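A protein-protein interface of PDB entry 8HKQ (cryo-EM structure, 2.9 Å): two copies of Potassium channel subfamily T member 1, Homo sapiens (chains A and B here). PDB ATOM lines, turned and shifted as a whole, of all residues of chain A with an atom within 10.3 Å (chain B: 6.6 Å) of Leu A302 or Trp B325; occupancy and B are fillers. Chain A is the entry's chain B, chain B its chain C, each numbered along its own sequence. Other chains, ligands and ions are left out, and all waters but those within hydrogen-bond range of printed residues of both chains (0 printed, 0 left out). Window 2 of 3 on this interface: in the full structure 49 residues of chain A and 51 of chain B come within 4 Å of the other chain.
No position is printed for both chains.
Of the 6 pairs that touch across the chains among the printed residues, none has its exchanged pair printed and touching as well.
Hydrophobic or aromatic side chains of chain B within 4 Å of the printed part of chain A: Trp B325, Leu B329 and Val B332.
Of the 25 printed residues of chain A, 4 touch a printed residue of chain B.
Among the printed residues, no Asp or Glu carboxylate lies within 4 Å of a Lys or Arg side-chain nitrogen of the other chain.
OG1 of Thr A286 lies within hydrogen-bond range of N of Phe A305 (2.9 Å).
The side-chain carboxylate (OD1) of Asp A319 is in hydrogen-bond range of the side-chain hydroxyl (OH) of Tyr A306, 3.4 Å away.
Leu A302 touches Trp B325 (CD2 to CE3, 3.4 Å).
CD1 of Leu B329 touches CD1 of Leu A302 (3.8 Å).
Phe A305 touches Val B332.
O of Gln B328 touches CD2 of Tyr A306, at 3.8 Å.
Val B332 touches Tyr A306 (CG2 to CD2, 3.7 Å).
Ile A309 touches Val B332.
Leu A302 touches just these residues of chain B: Trp B325 and Leu B329.
No residue of chain A comes within 4 Å of Ile B324.
No residue of chain A comes within 4 Å of Pro B326.
Gln B328 touches one residue of chain A.
Of chain A, only Leu A302 comes within 4 Å of Leu B329.
Printed residues of chain B within 4 Å of Ile A309: Val B332.
Of the printed residues of chain A, Val B332 touches Phe A305, Tyr A306 and Ile A309.
Val A134 touches none of the printed residues of chain B.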
ATOM      1  N   ILE A 131       4.739  10.708   6.378  1.00  0.00           N
ATOM      2  CA  ILE A 131       5.447   9.590   5.760  1.00  0.00           C
ATOM      3  C   ILE A 131       6.076   8.701   6.826  1.00  0.00           C
ATOM      4  O   ILE A 131       5.955   7.469   6.778  1.00  0.00           O
ATOM      5  CB  ILE A 131       6.504  10.105   4.765  1.00  0.00           C
ATOM      6  CG1 ILE A 131       5.910  10.258   3.368  1.00  0.00           C
ATOM      7  CG2 ILE A 131       7.702   9.170   4.709  1.00  0.00           C
ATOM      8  CD1 ILE A 131       6.766  11.099   2.454  1.00  0.00           C
ATOM      9  N   VAL A 134       3.409   6.634   8.502  1.00  0.00           N
ATOM     10  CA  VAL A 134       2.837   5.522   7.747  1.00  0.00           C
ATOM     11  C   VAL A 134       3.881   4.437   7.505  1.00  0.00           C
ATOM     12  O   VAL A 134       3.533   3.276   7.252  1.00  0.00           O
ATOM     13  CB  VAL A 134       2.215   6.022   6.428  1.00  0.00           C
ATOM     14  CG1 VAL A 134       3.294   6.416   5.427  1.00  0.00           C
ATOM     15  CG2 VAL A 134       1.262   4.979   5.848  1.00  0.00           C
ATOM     16  N   LEU A 135       5.169   4.782   7.583  1.00  0.00           N
ATOM     17  CA  LEU A 135       6.219   3.801   7.334  1.00  0.00           C
ATOM     18  C   LEU A 135       6.507   2.934   8.555  1.00  0.00           C
ATOM     19  O   LEU A 135       6.914   1.776   8.404  1.00  0.00           O
ATOM     20  CB  LEU A 135       7.491   4.515   6.857  1.00  0.00           C
ATOM     21  CG  LEU A 135       8.871   3.844   6.864  1.00  0.00           C
ATOM     22  CD1 LEU A 135       9.747   4.481   5.801  1.00  0.00           C
ATOM     23  CD2 LEU A 135       9.565   3.967   8.219  1.00  0.00           C
ATOM     24  N   VAL A 282       2.306  13.060  -7.573  1.00  0.00           N
ATOM     25  CA  VAL A 282       2.768  11.695  -7.335  1.00  0.00           C
ATOM     26  C   VAL A 282       2.709  11.368  -5.846  1.00  0.00           C
ATOM     27  O   VAL A 282       2.280  10.277  -5.450  1.00  0.00           O
ATOM     28  CB  VAL A 282       4.185  11.508  -7.911  1.00  0.00           C
ATOM     29  CG1 VAL A 282       4.949  10.449  -7.136  1.00  0.00           C
ATOM     30  CG2 VAL A 282       4.112  11.147  -9.387  1.00  0.00           C
ATOM     31  N   GLY A 285      -0.954  11.016  -4.671  1.00  0.00           N
ATOM     32  CA  GLY A 285      -1.462   9.787  -5.239  1.00  0.00           C
ATOM     33  C   GLY A 285      -0.973   8.551  -4.519  1.00  0.00           C
ATOM     34  O   GLY A 285      -1.774   7.669  -4.200  1.00  0.00           O
ATOM     35  N   THR A 286       0.335   8.465  -4.255  1.00  0.00           N
ATOM     36  CA  THR A 286       0.857   7.269  -3.601  1.00  0.00           C
ATOM     37  C   THR A 286       0.359   7.170  -2.163  1.00  0.00           C
ATOM     38  O   THR A 286       0.007   6.079  -1.695  1.00  0.00           O
ATOM     39  CB  THR A 286       2.390   7.227  -3.662  1.00  0.00           C
ATOM     40  OG1 THR A 286       2.857   6.046  -2.996  1.00  0.00           O
ATOM     41  CG2 THR A 286       3.021   8.439  -3.004  1.00  0.00           C
ATOM     42  N   CYS A 287       0.295   8.300  -1.448  1.00  0.00           N
ATOM     43  CA  CYS A 287      -0.224   8.250  -0.084  1.00  0.00           C
ATOM     44  C   CYS A 287      -1.679   7.804  -0.059  1.00  0.00           C
ATOM     45  O   CYS A 287      -2.051   6.930   0.736  1.00  0.00           O
ATOM     46  CB  CYS A 287      -0.067   9.603   0.607  1.00  0.00           C
ATOM     47  SG  CYS A 287       1.614  10.225   0.623  1.00  0.00           S
ATOM     48  N   ILE A 289      -3.331   6.059  -2.369  1.00  0.00           N
ATOM     49  CA  ILE A 289      -3.446   4.676  -2.811  1.00  0.00           C
ATOM     50  C   ILE A 289      -3.053   3.727  -1.692  1.00  0.00           C
ATOM     51  O   ILE A 289      -3.787   2.781  -1.390  1.00  0.00           O
ATOM     52  CB  ILE A 289      -2.596   4.441  -4.072  1.00  0.00           C
ATOM     53  CG1 ILE A 289      -3.366   4.876  -5.317  1.00  0.00           C
ATOM     54  CG2 ILE A 289      -2.217   2.972  -4.192  1.00  0.00           C
ATOM     55  CD1 ILE A 289      -4.700   4.186  -5.479  1.00  0.00           C
ATOM     56  N   GLN A 290      -1.924   3.985  -1.026  1.00  0.00           N
ATOM     57  CA  GLN A 290      -1.499   3.114   0.062  1.00  0.00           C
ATOM     58  C   GLN A 290      -2.511   3.120   1.200  1.00  0.00           C
ATOM     59  O   GLN A 290      -2.818   2.070   1.779  1.00  0.00           O
ATOM     60  CB  GLN A 290      -0.118   3.540   0.563  1.00  0.00           C
ATOM     61  CG  GLN A 290       0.553   2.543   1.497  1.00  0.00           C
ATOM     62  CD  GLN A 290       0.118   2.709   2.938  1.00  0.00           C
ATOM     63  OE1 GLN A 290      -0.411   3.754   3.321  1.00  0.00           O
ATOM     64  NE2 GLN A 290       0.339   1.680   3.747  1.00  0.00           N
ATOM     65  N   HIS A 291      -3.043   4.297   1.543  1.00  0.00           N
ATOM     66  CA  HIS A 291      -3.895   4.367   2.723  1.00  0.00           C
ATOM     67  C   HIS A 291      -5.245   3.699   2.486  1.00  0.00           C
ATOM     68  O   HIS A 291      -5.702   2.914   3.323  1.00  0.00           O
ATOM     69  CB  HIS A 291      -4.096   5.811   3.165  1.00  0.00           C
ATOM     70  CG  HIS A 291      -4.920   5.930   4.405  1.00  0.00           C
ATOM     71  ND1 HIS A 291      -4.705   5.134   5.510  1.00  0.00           N
ATOM     72  CD2 HIS A 291      -5.978   6.716   4.707  1.00  0.00           C
ATOM     73  CE1 HIS A 291      -5.582   5.440   6.447  1.00  0.00           C
ATOM     74  NE2 HIS A 291      -6.368   6.394   5.984  1.00  0.00           N
ATOM     75  N   ASN A 298      -3.374  -4.719   1.302  1.00  0.00           N
ATOM     76  CA  ASN A 298      -2.352  -4.454   2.324  1.00  0.00           C
ATOM     77  C   ASN A 298      -0.983  -4.137   1.715  1.00  0.00           C
ATOM     78  O   ASN A 298       0.045  -4.687   2.117  1.00  0.00           O
ATOM     79  CB  ASN A 298      -2.253  -5.625   3.302  1.00  0.00           C
ATOM     80  CG  ASN A 298      -2.626  -5.234   4.718  1.00  0.00           C
ATOM     81  OD1 ASN A 298      -3.473  -4.367   4.931  1.00  0.00           O
ATOM     82  ND2 ASN A 298      -1.994  -5.872   5.696  1.00  0.00           N
ATOM     83  N   LEU A 299      -0.973  -3.239   0.734  1.00  0.00           N
ATOM     84  CA  LEU A 299       0.244  -2.974  -0.018  1.00  0.00           C
ATOM     85  C   LEU A 299       1.095  -1.901   0.656  1.00  0.00           C
ATOM     86  O   LEU A 299       0.584  -0.956   1.264  1.00  0.00           O
ATOM     87  CB  LEU A 299      -0.093  -2.578  -1.459  1.00  0.00           C
ATOM     88  CG  LEU A 299      -0.931  -1.332  -1.768  1.00  0.00           C
ATOM     89  CD1 LEU A 299      -0.103  -0.056  -1.791  1.00  0.00           C
ATOM     90  CD2 LEU A 299      -1.667  -1.512  -3.090  1.00  0.00           C
ATOM     91  N   SER A 300       2.412  -2.062   0.537  1.00  0.00           N
ATOM     92  CA  SER A 300       3.364  -1.163   1.172  1.00  0.00           C
ATOM     93  C   SER A 300       3.447   0.164   0.416  1.00  0.00           C
ATOM     94  O   SER A 300       2.943   0.314  -0.701  1.00  0.00           O
ATOM     95  CB  SER A 300       4.745  -1.814   1.247  1.00  0.00           C
ATOM     96  OG  SER A 300       5.254  -2.074  -0.049  1.00  0.00           O
ATOM     97  N   LEU A 301       4.106   1.139   1.051  1.00  0.00           N
ATOM     98  CA  LEU A 301       4.180   2.482   0.484  1.00  0.00           C
ATOM     99  C   LEU A 301       5.012   2.521  -0.793  1.00  0.00           C
ATOM    100  O   LEU A 301       4.654   3.236  -1.735  1.00  0.00           O
ATOM    101  CB  LEU A 301       4.735   3.457   1.530  1.00  0.00           C
ATOM    102  CG  LEU A 301       5.259   4.849   1.146  1.00  0.00           C
ATOM    103  CD1 LEU A 301       5.140   5.772   2.342  1.00  0.00           C
ATOM    104  CD2 LEU A 301       6.710   4.831   0.672  1.00  0.00           C
ATOM    105  N   LEU A 302       6.126   1.784  -0.845  1.00  0.00           N
ATOM    106  CA  LEU A 302       6.958   1.801  -2.045  1.00  0.00           C
ATOM    107  C   LEU A 302       6.213   1.175  -3.217  1.00  0.00           C
ATOM    108  O   LEU A 302       6.326   1.635  -4.359  1.00  0.00           O
ATOM    109  CB  LEU A 302       8.279   1.072  -1.786  1.00  0.00           C
ATOM    110  CG  LEU A 302       9.099   0.504  -2.955  1.00  0.00           C
ATOM    111  CD1 LEU A 302       9.341   1.521  -4.069  1.00  0.00           C
ATOM    112  CD2 LEU A 302      10.418  -0.027  -2.465  1.00  0.00           C
ATOM    113  N   THR A 303       5.451   0.113  -2.953  1.00  0.00           N
ATOM    114  CA  THR A 303       4.627  -0.470  -4.004  1.00  0.00           C
ATOM    115  C   THR A 303       3.594   0.529  -4.505  1.00  0.00           C
ATOM    116  O   THR A 303       3.343   0.609  -5.713  1.00  0.00           O
ATOM    117  CB  THR A 303       3.943  -1.740  -3.495  1.00  0.00           C
ATOM    118  OG1 THR A 303       4.937  -2.672  -3.054  1.00  0.00           O
ATOM    119  CG2 THR A 303       3.120  -2.380  -4.600  1.00  0.00           C
ATOM    120  N   SER A 304       3.005   1.314  -3.599  1.00  0.00           N
ATOM    121  CA  SER A 304       2.083   2.366  -4.011  1.00  0.00           C
ATOM    122  C   SER A 304       2.780   3.414  -4.869  1.00  0.00           C
ATOM    123  O   SER A 304       2.223   3.868  -5.873  1.00  0.00           O
ATOM    124  CB  SER A 304       1.452   3.021  -2.784  1.00  0.00           C
ATOM    125  OG  SER A 304       0.583   4.071  -3.164  1.00  0.00           O
ATOM    126  N   PHE A 305       3.994   3.815  -4.485  1.00  0.00           N
ATOM    127  CA  PHE A 305       4.742   4.797  -5.266  1.00  0.00           C
ATOM    128  C   PHE A 305       5.059   4.273  -6.661  1.00  0.00           C
ATOM    129  O   PHE A 305       4.906   4.993  -7.655  1.00  0.00           O
ATOM    130  CB  PHE A 305       6.029   5.170  -4.530  1.00  0.00           C
ATOM    131  CG  PHE A 305       6.947   6.057  -5.320  1.00  0.00           C
ATOM    132  CD1 PHE A 305       8.146   5.565  -5.810  1.00  0.00           C
ATOM    133  CD2 PHE A 305       6.623   7.380  -5.564  1.00  0.00           C
ATOM    134  CE1 PHE A 305       8.999   6.374  -6.534  1.00  0.00           C
ATOM    135  CE2 PHE A 305       7.475   8.194  -6.287  1.00  0.00           C
ATOM    136  CZ  PHE A 305       8.664   7.690  -6.772  1.00  0.00           C
ATOM    137  N   TYR A 306       5.511   3.021  -6.748  1.00  0.00           N
ATOM    138  CA  TYR A 306       5.815   2.414  -8.040  1.00  0.00           C
ATOM    139  C   TYR A 306       4.565   2.301  -8.904  1.00  0.00           C
ATOM    140  O   TYR A 306       4.599   2.594 -10.105  1.00  0.00           O
ATOM    141  CB  TYR A 306       6.462   1.047  -7.816  1.00  0.00           C
ATOM    142  CG  TYR A 306       6.270   0.050  -8.934  1.00  0.00           C
ATOM    143  CD1 TYR A 306       5.299  -0.938  -8.845  1.00  0.00           C
ATOM    144  CD2 TYR A 306       7.071   0.082 -10.067  1.00  0.00           C
ATOM    145  CE1 TYR A 306       5.121  -1.858  -9.855  1.00  0.00           C
ATOM    146  CE2 TYR A 306       6.901  -0.836 -11.085  1.00  0.00           C
ATOM    147  CZ  TYR A 306       5.924  -1.803 -10.972  1.00  0.00           C
ATOM    148  OH  TYR A 306       5.748  -2.720 -11.979  1.00  0.00           O
ATOM    149  N   PHE A 307       3.449   1.890  -8.302  1.00  0.00           N
ATOM    150  CA  PHE A 307       2.185   1.808  -9.025  1.00  0.00           C
ATOM    151  C   PHE A 307       1.759   3.182  -9.530  1.00  0.00           C
ATOM    152  O   PHE A 307       1.319   3.332 -10.678  1.00  0.00           O
ATOM    153  CB  PHE A 307       1.135   1.187  -8.099  1.00  0.00           C
ATOM    154  CG  PHE A 307      -0.275   1.578  -8.407  1.00  0.00           C
ATOM    155  CD1 PHE A 307      -0.973   0.957  -9.426  1.00  0.00           C
ATOM    156  CD2 PHE A 307      -0.918   2.547  -7.655  1.00  0.00           C
ATOM    157  CE1 PHE A 307      -2.277   1.302  -9.698  1.00  0.00           C
ATOM    158  CE2 PHE A 307      -2.222   2.901  -7.928  1.00  0.00           C
ATOM    159  CZ  PHE A 307      -2.903   2.278  -8.950  1.00  0.00           C
ATOM    160  N   CYS A 308       1.919   4.209  -8.692  1.00  0.00           N
ATOM    161  CA  CYS A 308       1.527   5.560  -9.069  1.00  0.00           C
ATOM    162  C   CYS A 308       2.398   6.119 -10.186  1.00  0.00           C
ATOM    163  O   CYS A 308       1.891   6.820 -11.068  1.00  0.00           O
ATOM    164  CB  CYS A 308       1.580   6.476  -7.849  1.00  0.00           C
ATOM    165  SG  CYS A 308      -0.007   6.666  -7.023  1.00  0.00           S
ATOM    166  N   ILE A 309       3.701   5.840 -10.168  1.00  0.00           N
ATOM    167  CA  ILE A 309       4.544   6.369 -11.235  1.00  0.00           C
ATOM    168  C   ILE A 309       4.333   5.592 -12.533  1.00  0.00           C
ATOM    169  O   ILE A 309       4.384   6.176 -13.621  1.00  0.00           O
ATOM    170  CB  ILE A 309       6.026   6.394 -10.820  1.00  0.00           C
ATOM    171  CG1 ILE A 309       6.912   6.810 -11.996  1.00  0.00           C
ATOM    172  CG2 ILE A 309       6.467   5.045 -10.344  1.00  0.00           C
ATOM    173  CD1 ILE A 309       6.763   8.261 -12.389  1.00  0.00           C
ATOM    174  N   VAL A 310       4.084   4.279 -12.463  1.00  0.00           N
ATOM    175  CA  VAL A 310       3.834   3.549 -13.703  1.00  0.00           C
ATOM    176  C   VAL A 310       2.459   3.858 -14.283  1.00  0.00           C
ATOM    177  O   VAL A 310       2.270   3.720 -15.498  1.00  0.00           O
ATOM    178  CB  VAL A 310       3.993   2.028 -13.530  1.00  0.00           C
ATOM    179  CG1 VAL A 310       5.401   1.689 -13.064  1.00  0.00           C
ATOM    180  CG2 VAL A 310       2.945   1.472 -12.585  1.00  0.00           C
ATOM    181  N   ASP A 319       0.205  -5.340 -12.611  1.00  0.00           N
ATOM    182  CA  ASP A 319       0.634  -6.320 -11.616  1.00  0.00           C
ATOM    183  C   ASP A 319       0.091  -5.973 -10.236  1.00  0.00           C
ATOM    184  O   ASP A 319      -0.387  -6.852  -9.510  1.00  0.00           O
ATOM    185  CB  ASP A 319       2.158  -6.408 -11.583  1.00  0.00           C
ATOM    186  CG  ASP A 319       2.814  -5.084 -11.239  1.00  0.00           C
ATOM    187  OD1 ASP A 319       2.598  -4.102 -11.979  1.00  0.00           O
ATOM    188  OD2 ASP A 319       3.544  -5.026 -10.228  1.00  0.00           O
ATOM    189  N   VAL A 320       0.153  -4.699  -9.862  1.00  0.00           N
ATOM    190  CA  VAL A 320      -0.448  -4.193  -8.635  1.00  0.00           C
ATOM    191  C   VAL A 320      -1.544  -3.219  -9.037  1.00  0.00           C
ATOM    192  O   VAL A 320      -1.270  -2.200  -9.680  1.00  0.00           O
ATOM    193  CB  VAL A 320       0.591  -3.512  -7.726  1.00  0.00           C
ATOM    194  CG1 VAL A 320      -0.094  -2.862  -6.533  1.00  0.00           C
ATOM    195  CG2 VAL A 320       1.637  -4.518  -7.270  1.00  0.00           C
ATOM    196  N   ILE B 162      15.229 -10.556  -0.117  1.00  0.00           N
ATOM    197  CA  ILE B 162      15.783 -10.533  -1.464  1.00  0.00           C
ATOM    198  C   ILE B 162      17.207 -11.047  -1.388  1.00  0.00           C
ATOM    199  O   ILE B 162      18.059 -10.456  -0.712  1.00  0.00           O
ATOM    200  CB  ILE B 162      15.757  -9.129  -2.081  1.00  0.00           C
ATOM    201  CG1 ILE B 162      14.322  -8.661  -2.290  1.00  0.00           C
ATOM    202  CG2 ILE B 162      16.508  -9.125  -3.415  1.00  0.00           C
ATOM    203  CD1 ILE B 162      14.226  -7.204  -2.588  1.00  0.00           C
ATOM    204  N   TRP B 164      20.817 -11.443  -2.739  1.00  0.00           N
ATOM    205  CA  TRP B 164      21.679 -10.588  -3.543  1.00  0.00           C
ATOM    206  C   TRP B 164      22.833 -11.339  -4.192  1.00  0.00           C
ATOM    207  O   TRP B 164      23.514 -10.766  -5.044  1.00  0.00           O
ATOM    208  CB  TRP B 164      22.239  -9.440  -2.697  1.00  0.00           C
ATOM    209  CG  TRP B 164      21.231  -8.697  -1.869  1.00  0.00           C
ATOM    210  CD1 TRP B 164      20.723  -9.081  -0.663  1.00  0.00           C
ATOM    211  CD2 TRP B 164      20.652  -7.415  -2.159  1.00  0.00           C
ATOM    212  NE1 TRP B 164      19.844  -8.132  -0.195  1.00  0.00           N
ATOM    213  CE2 TRP B 164      19.784  -7.098  -1.094  1.00  0.00           C
ATOM    214  CE3 TRP B 164      20.775  -6.513  -3.220  1.00  0.00           C
ATOM    215  CZ2 TRP B 164      19.044  -5.915  -1.059  1.00  0.00           C
ATOM    216  CZ3 TRP B 164      20.037  -5.337  -3.182  1.00  0.00           C
ATOM    217  CH2 TRP B 164      19.184  -5.051  -2.110  1.00  0.00           C
ATOM    218  N   LEU B 292      19.055  -7.224 -13.043  1.00  0.00           N
ATOM    219  CA  LEU B 292      18.380  -7.144 -11.751  1.00  0.00           C
ATOM    220  C   LEU B 292      17.306  -8.217 -11.622  1.00  0.00           C
ATOM    221  O   LEU B 292      16.889  -8.556 -10.508  1.00  0.00           O
ATOM    222  CB  LEU B 292      17.786  -5.749 -11.553  1.00  0.00           C
ATOM    223  CG  LEU B 292      18.687  -4.708 -10.882  1.00  0.00           C
ATOM    224  CD1 LEU B 292      19.763  -4.198 -11.825  1.00  0.00           C
ATOM    225  CD2 LEU B 292      17.848  -3.552 -10.368  1.00  0.00           C
ATOM    226  N   LYS B 323       8.693  -8.133 -10.157  1.00  0.00           N
ATOM    227  CA  LYS B 323       8.055  -8.446  -8.885  1.00  0.00           C
ATOM    228  C   LYS B 323       8.999  -8.262  -7.705  1.00  0.00           C
ATOM    229  O   LYS B 323       8.703  -8.745  -6.606  1.00  0.00           O
ATOM    230  CB  LYS B 323       7.506  -9.877  -8.895  1.00  0.00           C
ATOM    231  CG  LYS B 323       6.391 -10.126  -9.902  1.00  0.00           C
ATOM    232  CD  LYS B 323       5.839 -11.541  -9.763  1.00  0.00           C
ATOM    233  CE  LYS B 323       5.856 -12.314 -11.075  1.00  0.00           C
ATOM    234  NZ  LYS B 323       5.417 -11.500 -12.245  1.00  0.00           N
ATOM    235  N   ILE B 324      10.123  -7.571  -7.897  1.00  0.00           N
ATOM    236  CA  ILE B 324      11.144  -7.432  -6.870  1.00  0.00           C
ATOM    237  C   ILE B 324      11.486  -5.955  -6.709  1.00  0.00           C
ATOM    238  O   ILE B 324      11.285  -5.140  -7.612  1.00  0.00           O
ATOM    239  CB  ILE B 324      12.405  -8.277  -7.188  1.00  0.00           C
ATOM    240  CG1 ILE B 324      13.303  -7.584  -8.210  1.00  0.00           C
ATOM    241  CG2 ILE B 324      12.032  -9.676  -7.674  1.00  0.00           C
ATOM    242  CD1 ILE B 324      14.768  -7.874  -8.008  1.00  0.00           C
ATOM    243  N   TRP B 325      11.985  -5.618  -5.520  1.00  0.00           N
ATOM    244  CA  TRP B 325      12.261  -4.259  -5.058  1.00  0.00           C
ATOM    245  C   TRP B 325      13.214  -3.526  -6.008  1.00  0.00           C
ATOM    246  O   TRP B 325      12.830  -2.490  -6.577  1.00  0.00           O
ATOM    247  CB  TRP B 325      12.814  -4.340  -3.625  1.00  0.00           C
ATOM    248  CG  TRP B 325      13.635  -3.189  -3.095  1.00  0.00           C
ATOM    249  CD1 TRP B 325      14.870  -2.785  -3.522  1.00  0.00           C
ATOM    250  CD2 TRP B 325      13.359  -2.424  -1.914  1.00  0.00           C
ATOM    251  NE1 TRP B 325      15.325  -1.748  -2.748  1.00  0.00           N
ATOM    252  CE2 TRP B 325      14.422  -1.515  -1.745  1.00  0.00           C
ATOM    253  CE3 TRP B 325      12.296  -2.396  -1.004  1.00  0.00           C
ATOM    254  CZ2 TRP B 325      14.451  -0.584  -0.707  1.00  0.00           C
ATOM    255  CZ3 TRP B 325      12.327  -1.468   0.025  1.00  0.00           C
ATOM    256  CH2 TRP B 325      13.397  -0.575   0.164  1.00  0.00           C
ATOM    257  N   PRO B 326      14.451  -4.009  -6.215  1.00  0.00           N
ATOM    258  CA  PRO B 326      15.375  -3.230  -7.054  1.00  0.00           C
ATOM    259  C   PRO B 326      14.898  -3.084  -8.484  1.00  0.00           C
ATOM    260  O   PRO B 326      15.127  -2.035  -9.092  1.00  0.00           O
ATOM    261  CB  PRO B 326      16.701  -4.005  -6.974  1.00  0.00           C
ATOM    262  CG  PRO B 326      16.484  -5.155  -6.112  1.00  0.00           C
ATOM    263  CD  PRO B 326      15.046  -5.287  -5.777  1.00  0.00           C
ATOM    264  N   SER B 327      14.234  -4.099  -9.043  1.00  0.00           N
ATOM    265  CA  SER B 327      13.799  -3.997 -10.433  1.00  0.00           C
ATOM    266  C   SER B 327      12.646  -3.014 -10.591  1.00  0.00           C
ATOM    267  O   SER B 327      12.608  -2.257 -11.569  1.00  0.00           O
ATOM    268  CB  SER B 327      13.405  -5.372 -10.971  1.00  0.00           C
ATOM    269  OG  SER B 327      13.007  -5.293 -12.329  1.00  0.00           O
ATOM    270  N   GLN B 328      11.703  -3.002  -9.645  1.00  0.00           N
ATOM    271  CA  GLN B 328      10.634  -2.010  -9.681  1.00  0.00           C
ATOM    272  C   GLN B 328      11.195  -0.601  -9.538  1.00  0.00           C
ATOM    273  O   GLN B 328      10.815   0.314 -10.282  1.00  0.00           O
ATOM    274  CB  GLN B 328       9.612  -2.302  -8.582  1.00  0.00           C
ATOM    275  CG  GLN B 328       8.762  -3.532  -8.840  1.00  0.00           C
ATOM    276  CD  GLN B 328       7.902  -3.899  -7.650  1.00  0.00           C
ATOM    277  OE1 GLN B 328       8.096  -3.386  -6.549  1.00  0.00           O
ATOM    278  NE2 GLN B 328       6.944  -4.793  -7.865  1.00  0.00           N
ATOM    279  N   LEU B 329      12.121  -0.410  -8.594  1.00  0.00           N
ATOM    280  CA  LEU B 329      12.733   0.905  -8.450  1.00  0.00           C
ATOM    281  C   LEU B 329      13.531   1.300  -9.685  1.00  0.00           C
ATOM    282  O   LEU B 329      13.559   2.484 -10.037  1.00  0.00           O
ATOM    283  CB  LEU B 329      13.629   0.941  -7.212  1.00  0.00           C
ATOM    284  CG  LEU B 329      13.717   2.301  -6.519  1.00  0.00           C
ATOM    285  CD1 LEU B 329      12.350   2.711  -5.991  1.00  0.00           C
ATOM    286  CD2 LEU B 329      14.742   2.267  -5.400  1.00  0.00           C
ATOM    287  N   LEU B 330      14.173   0.334 -10.347  1.00  0.00           N
ATOM    288  CA  LEU B 330      14.905   0.614 -11.576  1.00  0.00           C
ATOM    289  C   LEU B 330      13.956   1.050 -12.683  1.00  0.00           C
ATOM    290  O   LEU B 330      14.252   1.986 -13.432  1.00  0.00           O
ATOM    291  CB  LEU B 330      15.702  -0.620 -11.998  1.00  0.00           C
ATOM    292  CG  LEU B 330      16.209  -0.743 -13.438  1.00  0.00           C
ATOM    293  CD1 LEU B 330      17.017   0.479 -13.875  1.00  0.00           C
ATOM    294  CD2 LEU B 330      17.024  -2.008 -13.588  1.00  0.00           C
ATOM    295  N   VAL B 332      11.195   2.572 -12.161  1.00  0.00           N
ATOM    296  CA  VAL B 332      10.758   3.910 -11.770  1.00  0.00           C
ATOM    297  C   VAL B 332      11.788   4.959 -12.185  1.00  0.00           C
ATOM    298  O   VAL B 332      11.453   5.966 -12.827  1.00  0.00           O
ATOM    299  CB  VAL B 332      10.493   3.956 -10.255  1.00  0.00           C
ATOM    300  CG1 VAL B 332      10.294   5.389  -9.788  1.00  0.00           C
ATOM    301  CG2 VAL B 332       9.304   3.083  -9.895  1.00  0.00           C
